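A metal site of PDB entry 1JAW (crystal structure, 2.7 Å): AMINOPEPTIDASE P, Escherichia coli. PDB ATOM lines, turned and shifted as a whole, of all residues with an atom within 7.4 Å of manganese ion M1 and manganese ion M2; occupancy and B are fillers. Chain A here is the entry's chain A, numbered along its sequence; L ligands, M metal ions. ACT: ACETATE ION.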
ATOM      1  N   TYR A 229       4.767   4.172 -31.558  1.00  0.00           N
ATOM      2  CA  TYR A 229       5.222   4.493 -32.913  1.00  0.00           C
ATOM      3  C   TYR A 229       4.851   3.308 -33.798  1.00  0.00           C
ATOM      4  O   TYR A 229       4.510   2.227 -33.298  1.00  0.00           O
ATOM      5  CB  TYR A 229       6.748   4.704 -32.963  1.00  0.00           C
ATOM      6  CG  TYR A 229       7.544   3.543 -32.411  1.00  0.00           C
ATOM      7  CD1 TYR A 229       7.823   3.460 -31.057  1.00  0.00           C
ATOM      8  CD2 TYR A 229       7.985   2.496 -33.232  1.00  0.00           C
ATOM      9  CE1 TYR A 229       8.506   2.389 -30.509  1.00  0.00           C
ATOM     10  CE2 TYR A 229       8.671   1.402 -32.688  1.00  0.00           C
ATOM     11  CZ  TYR A 229       8.926   1.365 -31.332  1.00  0.00           C
ATOM     12  OH  TYR A 229       9.608   0.313 -30.771  1.00  0.00           O
ATOM     13  N   ILE A 232       7.851  -1.886 -36.697  1.00  0.00           N
ATOM     14  CA  ILE A 232       8.772  -2.324 -37.738  1.00  0.00           C
ATOM     15  C   ILE A 232       8.932  -3.840 -37.675  1.00  0.00           C
ATOM     16  O   ILE A 232       9.273  -4.383 -36.613  1.00  0.00           O
ATOM     17  CB  ILE A 232      10.204  -1.753 -37.536  1.00  0.00           C
ATOM     18  CG1 ILE A 232      10.205  -0.261 -37.202  1.00  0.00           C
ATOM     19  CG2 ILE A 232      11.036  -2.018 -38.768  1.00  0.00           C
ATOM     20  CD1 ILE A 232       9.788   0.619 -38.330  1.00  0.00           C
ATOM     21  N   HIS A 243      13.357   2.282 -40.760  1.00  0.00           N
ATOM     22  CA  HIS A 243      11.950   2.346 -40.406  1.00  0.00           C
ATOM     23  C   HIS A 243      11.129   1.710 -41.546  1.00  0.00           C
ATOM     24  O   HIS A 243      10.521   2.391 -42.370  1.00  0.00           O
ATOM     25  CB  HIS A 243      11.488   3.805 -40.124  1.00  0.00           C
ATOM     26  CG  HIS A 243      12.190   4.470 -38.976  1.00  0.00           C
ATOM     27  ND1 HIS A 243      12.446   5.829 -38.961  1.00  0.00           N
ATOM     28  CD2 HIS A 243      12.669   3.994 -37.805  1.00  0.00           C
ATOM     29  CE1 HIS A 243      13.064   6.150 -37.833  1.00  0.00           C
ATOM     30  NE2 HIS A 243      13.209   5.051 -37.106  1.00  0.00           N
ATOM     31  N   ILE A 259      12.403  -6.767 -35.383  1.00  0.00           N
ATOM     32  CA  ILE A 259      11.172  -6.174 -34.879  1.00  0.00           C
ATOM     33  C   ILE A 259      11.446  -4.948 -34.012  1.00  0.00           C
ATOM     34  O   ILE A 259      12.061  -5.070 -32.954  1.00  0.00           O
ATOM     35  CB  ILE A 259      10.355  -7.178 -34.073  1.00  0.00           C
ATOM     36  CG1 ILE A 259      10.008  -8.391 -34.949  1.00  0.00           C
ATOM     37  CG2 ILE A 259       9.110  -6.523 -33.534  1.00  0.00           C
ATOM     38  CD1 ILE A 259       9.103  -9.381 -34.297  1.00  0.00           C
ATOM     39  N   ASP A 260      10.925  -3.699 -34.570  1.00  0.00           N
ATOM     40  CA  ASP A 260      11.218  -2.586 -33.709  1.00  0.00           C
ATOM     41  C   ASP A 260       9.552  -2.035 -33.186  1.00  0.00           C
ATOM     42  O   ASP A 260       8.870  -1.769 -34.069  1.00  0.00           O
ATOM     43  CB  ASP A 260      11.949  -1.517 -34.165  1.00  0.00           C
ATOM     44  CG  ASP A 260      12.350  -0.459 -33.185  1.00  0.00           C
ATOM     45  OD1 ASP A 260      12.100  -0.572 -31.954  1.00  0.00           O
ATOM     46  OD2 ASP A 260      12.870   0.576 -33.527  1.00  0.00           O
ATOM     47  N   ALA A 261       9.245  -2.395 -32.065  1.00  0.00           N
ATOM     48  CA  ALA A 261       7.886  -2.142 -31.597  1.00  0.00           C
ATOM     49  C   ALA A 261       7.840  -1.730 -30.129  1.00  0.00           C
ATOM     50  O   ALA A 261       8.558  -2.282 -29.284  1.00  0.00           O
ATOM     51  CB  ALA A 261       7.011  -3.365 -31.828  1.00  0.00           C
ATOM     52  N   GLY A 262       6.996  -0.729 -29.831  1.00  0.00           N
ATOM     53  CA  GLY A 262       6.846  -0.235 -28.467  1.00  0.00           C
ATOM     54  C   GLY A 262       5.425   0.169 -28.115  1.00  0.00           C
ATOM     55  O   GLY A 262       4.698   0.728 -28.939  1.00  0.00           O
ATOM     56  N   GLY A 270       7.361   2.713 -24.873  1.00  0.00           N
ATOM     57  CA  GLY A 270       8.193   1.551 -24.657  1.00  0.00           C
ATOM     58  C   GLY A 270       8.991   1.310 -25.935  1.00  0.00           C
ATOM     59  O   GLY A 270       8.633   1.819 -27.012  1.00  0.00           O
ATOM     60  N   ASP A 271      10.545   0.929 -26.129  1.00  0.00           N
ATOM     61  CA  ASP A 271      11.392   0.931 -27.527  1.00  0.00           C
ATOM     62  C   ASP A 271      11.967  -0.213 -27.373  1.00  0.00           C
ATOM     63  O   ASP A 271      13.020  -0.180 -26.785  1.00  0.00           O
ATOM     64  CB  ASP A 271      12.145   2.056 -27.509  1.00  0.00           C
ATOM     65  CG  ASP A 271      12.102   2.511 -28.854  1.00  0.00           C
ATOM     66  OD1 ASP A 271      11.656   1.662 -29.665  1.00  0.00           O
ATOM     67  OD2 ASP A 271      12.708   3.691 -29.321  1.00  0.00           O
ATOM     68  N   ILE A 272      11.430  -1.179 -28.039  1.00  0.00           N
ATOM     69  CA  ILE A 272      12.290  -2.354 -28.010  1.00  0.00           C
ATOM     70  C   ILE A 272      12.555  -2.903 -29.399  1.00  0.00           C
ATOM     71  O   ILE A 272      11.673  -2.948 -30.252  1.00  0.00           O
ATOM     72  CB  ILE A 272      11.642  -3.505 -27.186  1.00  0.00           C
ATOM     73  CG1 ILE A 272      11.759  -3.251 -25.667  1.00  0.00           C
ATOM     74  CG2 ILE A 272      12.323  -4.829 -27.467  1.00  0.00           C
ATOM     75  CD1 ILE A 272      11.315  -4.446 -24.823  1.00  0.00           C
ATOM     76  N   THR A 273      13.806  -3.299 -29.643  1.00  0.00           N
ATOM     77  CA  THR A 273      14.179  -3.903 -30.912  1.00  0.00           C
ATOM     78  C   THR A 273      14.842  -5.249 -30.637  1.00  0.00           C
ATOM     79  O   THR A 273      15.702  -5.355 -29.769  1.00  0.00           O
ATOM     80  CB  THR A 273      15.152  -3.062 -31.756  1.00  0.00           C
ATOM     81  OG1 THR A 273      14.670  -1.721 -31.862  1.00  0.00           O
ATOM     82  CG2 THR A 273      15.250  -3.647 -33.155  1.00  0.00           C
ATOM     83  N   LEU A 352      23.152   6.060 -31.246  1.00  0.00           N
ATOM     84  CA  LEU A 352      23.134   4.906 -30.354  1.00  0.00           C
ATOM     85  C   LEU A 352      22.007   5.006 -29.324  1.00  0.00           C
ATOM     86  O   LEU A 352      21.483   3.992 -28.837  1.00  0.00           O
ATOM     87  CB  LEU A 352      24.492   4.791 -29.619  1.00  0.00           C
ATOM     88  CG  LEU A 352      24.630   3.677 -28.580  1.00  0.00           C
ATOM     89  CD1 LEU A 352      24.791   2.351 -29.277  1.00  0.00           C
ATOM     90  CD2 LEU A 352      25.805   3.939 -27.669  1.00  0.00           C
ATOM     91  N   SER A 353      21.625   6.231 -29.002  1.00  0.00           N
ATOM     92  CA  SER A 353      20.596   6.471 -28.015  1.00  0.00           C
ATOM     93  C   SER A 353      19.750   7.696 -28.336  1.00  0.00           C
ATOM     94  O   SER A 353      20.256   8.816 -28.451  1.00  0.00           O
ATOM     95  CB  SER A 353      21.256   6.642 -26.645  1.00  0.00           C
ATOM     96  OG  SER A 353      21.949   5.470 -26.283  1.00  0.00           O
ATOM     97  N   HIS A 354      18.329   7.573 -27.919  1.00  0.00           N
ATOM     98  CA  HIS A 354      17.516   8.822 -27.895  1.00  0.00           C
ATOM     99  C   HIS A 354      16.813   8.721 -26.398  1.00  0.00           C
ATOM    100  O   HIS A 354      16.749   7.478 -25.772  1.00  0.00           O
ATOM    101  CB  HIS A 354      16.537   8.935 -29.086  1.00  0.00           C
ATOM    102  CG  HIS A 354      15.743   7.703 -29.194  1.00  0.00           C
ATOM    103  ND1 HIS A 354      14.612   7.489 -28.419  1.00  0.00           N
ATOM    104  CD2 HIS A 354      15.767   6.575 -29.954  1.00  0.00           C
ATOM    105  CE1 HIS A 354      14.019   6.294 -28.799  1.00  0.00           C
ATOM    106  NE2 HIS A 354      14.654   5.616 -29.801  1.00  0.00           N
ATOM    107  N   TRP A 355      16.605  10.118 -26.004  1.00  0.00           N
ATOM    108  CA  TRP A 355      15.752  10.291 -24.835  1.00  0.00           C
ATOM    109  C   TRP A 355      14.440   9.527 -25.026  1.00  0.00           C
ATOM    110  O   TRP A 355      13.941   9.407 -26.142  1.00  0.00           O
ATOM    111  CB  TRP A 355      15.428  11.767 -24.605  1.00  0.00           C
ATOM    112  CG  TRP A 355      16.609  12.701 -24.473  1.00  0.00           C
ATOM    113  CD1 TRP A 355      16.727  13.929 -25.043  1.00  0.00           C
ATOM    114  CD2 TRP A 355      17.779  12.515 -23.672  1.00  0.00           C
ATOM    115  NE1 TRP A 355      17.894  14.538 -24.643  1.00  0.00           N
ATOM    116  CE2 TRP A 355      18.565  13.685 -23.793  1.00  0.00           C
ATOM    117  CE3 TRP A 355      18.250  11.473 -22.854  1.00  0.00           C
ATOM    118  CZ2 TRP A 355      19.790  13.850 -23.121  1.00  0.00           C
ATOM    119  CZ3 TRP A 355      19.475  11.638 -22.182  1.00  0.00           C
ATOM    120  CH2 TRP A 355      20.230  12.814 -22.337  1.00  0.00           C
ATOM    121  N   LEU A 356      13.868   9.060 -23.917  1.00  0.00           N
ATOM    122  CA  LEU A 356      12.607   8.308 -23.945  1.00  0.00           C
ATOM    123  C   LEU A 356      11.640   8.824 -22.870  1.00  0.00           C
ATOM    124  O   LEU A 356      12.040   9.061 -21.723  1.00  0.00           O
ATOM    125  CB  LEU A 356      12.883   6.823 -23.698  1.00  0.00           C
ATOM    126  CG  LEU A 356      11.742   5.827 -23.838  1.00  0.00           C
ATOM    127  CD1 LEU A 356      11.304   5.674 -25.298  1.00  0.00           C
ATOM    128  CD2 LEU A 356      12.184   4.503 -23.268  1.00  0.00           C
ATOM    129  N   VAL A 360       8.414   8.740 -27.932  1.00  0.00           N
ATOM    130  CA  VAL A 360       9.537   7.782 -28.113  1.00  0.00           C
ATOM    131  C   VAL A 360      10.836   8.551 -28.245  1.00  0.00           C
ATOM    132  O   VAL A 360      11.816   8.227 -27.576  1.00  0.00           O
ATOM    133  CB  VAL A 360       9.458   6.938 -29.382  1.00  0.00           C
ATOM    134  CG1 VAL A 360       9.175   5.511 -29.021  1.00  0.00           C
ATOM    135  CG2 VAL A 360       8.475   7.503 -30.380  1.00  0.00           C
ATOM    136  N   HIS A 361      10.853   9.505 -29.165  1.00  0.00           N
ATOM    137  CA  HIS A 361      12.008  10.364 -29.351  1.00  0.00           C
ATOM    138  C   HIS A 361      11.633  11.575 -28.516  1.00  0.00           C
ATOM    139  O   HIS A 361      11.119  12.582 -29.018  1.00  0.00           O
ATOM    140  CB  HIS A 361      12.188  10.723 -30.824  1.00  0.00           C
ATOM    141  CG  HIS A 361      12.447   9.538 -31.704  1.00  0.00           C
ATOM    142  ND1 HIS A 361      12.221   9.551 -33.063  1.00  0.00           N
ATOM    143  CD2 HIS A 361      12.873   8.280 -31.403  1.00  0.00           C
ATOM    144  CE1 HIS A 361      12.494   8.357 -33.559  1.00  0.00           C
ATOM    145  NE2 HIS A 361      12.888   7.565 -32.580  1.00  0.00           N
ATOM    146  N   THR A 381      17.169   5.115 -24.757  1.00  0.00           N
ATOM    147  CA  THR A 381      17.222   3.815 -25.426  1.00  0.00           C
ATOM    148  C   THR A 381      18.702   3.488 -25.665  1.00  0.00           C
ATOM    149  O   THR A 381      19.550   4.375 -25.641  1.00  0.00           O
ATOM    150  CB  THR A 381      16.522   3.852 -26.795  1.00  0.00           C
ATOM    151  OG1 THR A 381      17.248   4.727 -27.670  1.00  0.00           O
ATOM    152  CG2 THR A 381      15.094   4.348 -26.648  1.00  0.00           C
ATOM    153  N   VAL A 382      19.014   2.206 -25.865  1.00  0.00           N
ATOM    154  CA  VAL A 382      20.389   1.781 -26.147  1.00  0.00           C
ATOM    155  C   VAL A 382      20.408   0.855 -27.361  1.00  0.00           C
ATOM    156  O   VAL A 382      19.767  -0.191 -27.379  1.00  0.00           O
ATOM    157  CB  VAL A 382      21.037   1.021 -24.970  1.00  0.00           C
ATOM    158  CG1 VAL A 382      22.490   0.693 -25.313  1.00  0.00           C
ATOM    159  CG2 VAL A 382      20.980   1.851 -23.685  1.00  0.00           C
ATOM    160  N   GLU A 383      20.528   1.584 -28.449  1.00  0.00           N
ATOM    161  CA  GLU A 383      20.142   0.692 -29.661  1.00  0.00           C
ATOM    162  C   GLU A 383      21.217   0.635 -30.895  1.00  0.00           C
ATOM    163  O   GLU A 383      20.978   1.449 -32.198  1.00  0.00           O
ATOM    164  CB  GLU A 383      18.884   1.237 -30.238  1.00  0.00           C
ATOM    165  CG  GLU A 383      18.796   2.658 -30.485  1.00  0.00           C
ATOM    166  CD  GLU A 383      17.564   3.106 -31.086  1.00  0.00           C
ATOM    167  OE1 GLU A 383      16.995   2.435 -31.928  1.00  0.00           O
ATOM    168  OE2 GLU A 383      17.053   4.168 -30.606  1.00  0.00           O
ATOM    169  N   ARG A 404      19.405  -5.045 -35.218  1.00  0.00           N
ATOM    170  CA  ARG A 404      19.340  -4.022 -34.175  1.00  0.00           C
ATOM    171  C   ARG A 404      18.866  -4.715 -32.901  1.00  0.00           C
ATOM    172  O   ARG A 404      18.081  -5.652 -32.960  1.00  0.00           O
ATOM    173  CB  ARG A 404      18.400  -2.861 -34.572  1.00  0.00           C
ATOM    174  CG  ARG A 404      18.312  -1.712 -33.551  1.00  0.00           C
ATOM    175  CD  ARG A 404      17.732  -0.420 -34.143  1.00  0.00           C
ATOM    176  NE  ARG A 404      16.335  -0.539 -34.604  1.00  0.00           N
ATOM    177  CZ  ARG A 404      15.949  -0.511 -35.880  1.00  0.00           C
ATOM    178  NH1 ARG A 404      16.838  -0.381 -36.855  1.00  0.00           N
ATOM    179  NH2 ARG A 404      14.666  -0.572 -36.188  1.00  0.00           N
ATOM    180  N   GLU A 406      17.628  -3.114 -29.241  1.00  0.00           N
ATOM    181  CA  GLU A 406      17.404  -1.799 -28.586  1.00  0.00           C
ATOM    182  C   GLU A 406      16.737  -2.171 -27.052  1.00  0.00           C
ATOM    183  O   GLU A 406      16.016  -3.087 -27.012  1.00  0.00           O
ATOM    184  CB  GLU A 406      16.410  -1.042 -29.389  1.00  0.00           C
ATOM    185  CG  GLU A 406      15.650  -0.397 -28.747  1.00  0.00           C
ATOM    186  CD  GLU A 406      15.225   0.772 -29.414  1.00  0.00           C
ATOM    187  OE1 GLU A 406      14.441   0.760 -30.610  1.00  0.00           O
ATOM    188  OE2 GLU A 406      15.447   2.081 -28.980  1.00  0.00           O
ATOM    189  N   ASP A 407      17.167  -1.867 -26.117  1.00  0.00           N
ATOM    190  CA  ASP A 407      16.802  -1.777 -24.714  1.00  0.00           C
ATOM    191  C   ASP A 407      16.586  -0.349 -24.245  1.00  0.00           C
ATOM    192  O   ASP A 407      17.185   0.595 -24.761  1.00  0.00           O
ATOM    193  CB  ASP A 407      17.857  -2.454 -23.836  1.00  0.00           C
ATOM    194  CG  ASP A 407      17.670  -3.960 -23.723  1.00  0.00           C
ATOM    195  OD1 ASP A 407      16.711  -4.500 -24.313  1.00  0.00           O
ATOM    196  OD2 ASP A 407      18.491  -4.599 -23.033  1.00  0.00           O
ATOM    197  N   ASP A 408      15.714  -0.190 -23.243  1.00  0.00           N
ATOM    198  CA  ASP A 408      15.397   1.114 -22.681  1.00  0.00           C
ATOM    199  C   ASP A 408      15.956   1.138 -21.271  1.00  0.00           C
ATOM    200  O   ASP A 408      15.789   0.174 -20.519  1.00  0.00           O
ATOM    201  CB  ASP A 408      13.883   1.329 -22.639  1.00  0.00           C
ATOM    202  CG  ASP A 408      13.223   1.031 -23.964  1.00  0.00           C
ATOM    203  OD1 ASP A 408      13.804   1.324 -25.037  1.00  0.00           O
ATOM    204  OD2 ASP A 408      12.100   0.486 -23.933  1.00  0.00           O
HETATM  205  C   ACT L   1      12.781   3.782 -32.967  1.00  0.00           C
HETATM  206  O   ACT L   1      13.807   3.428 -32.389  1.00  0.00           O
HETATM  207  OXT ACT L   1      12.747   5.028 -32.983  1.00  0.00           O
HETATM  208  CH3 ACT L   1      11.690   3.096 -33.490  1.00  0.00           C
HETATM  209 MN    MN M   1      14.615   3.679 -30.383  1.00  0.00          MN
HETATM  210 MN    MN M   2      13.111   1.439 -31.553  1.00  0.00          MN
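Residues that only touch manganese ion M1: Thr 381.
Five residues have an atom within 4 Å of manganese ion M1: Asp 271, His 354, Thr 381, Glu 383 and Glu 406.
The nearest printed residue that does not touch manganese ion M1 is Asp 260 (4.7 Å).
The side-chain hydroxyl of Thr 273 sits at hydrogen-bond distance from the guanidinium group of Arg 404 (3.4 Å).
The side-chain hydroxyl (OH) of Tyr 229 lies close to the side-chain carboxylate (OD1) of Asp 260 (2.9 Å).
The backbone carbonyl oxygen of His 354 is in hydrogen-bond range of the backbone NH of Thr 381 (2.6 Å).
N of Glu 383 is in hydrogen-bond range of O of Leu 352, at 2.6 Å.
N of Ala 261 sits close to OH of Tyr 229, at 3.0 Å.
The backbone NH (N) of Asp 260 is in hydrogen-bond range of the backbone carbonyl oxygen (O) of Ile 232 (2.7 Å).
N of Asp 271 sits at hydrogen-bond distance from OD2 of Asp 408 (2.7 Å).
The side-chain carboxylate (OE2) of Glu 406 lies close to the side-chain hydroxyl (OG1) of Thr 381, 3.5 Å away.
Manganese ion M2 is bound by the side-chain carboxylate (OE1) of Glu 406 (1.8 Å), the side-chain carboxylate (OD2) of Asp 260 (2.2 Å), an oxygen (O) of the ligand (2.3 Å), the side-chain carboxylate (OD1) of Asp 260 (2.3 Å) and the side-chain carboxylate (OD1) of Asp 271 (2.4 Å).
Manganese ion M1 is bound by NE2 of His 354 (2.0 Å), O of the ligand (2.2 Å), OD2 of Asp 271 (2.2 Å), OE2 of Glu 406 (2.3 Å) and OE2 of Glu 383 (2.5 Å).
Manganese ion M1 has five donor atoms within binding distance.
Slightly farther from manganese ion M1 lies OE1 of Glu 406 (2.9 Å).
Tyr 229 touches manganese ion M2 (OH to MN, 3.8 Å).
Thr 273 touches manganese ion M2.
Within 4 Å of manganese ion M2: Tyr 229, Asp 260, Asp 271, Thr 273 and Glu 406.
The nearest printed residue that does not touch manganese ion M2 is Glu 383 (4.03 Å).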
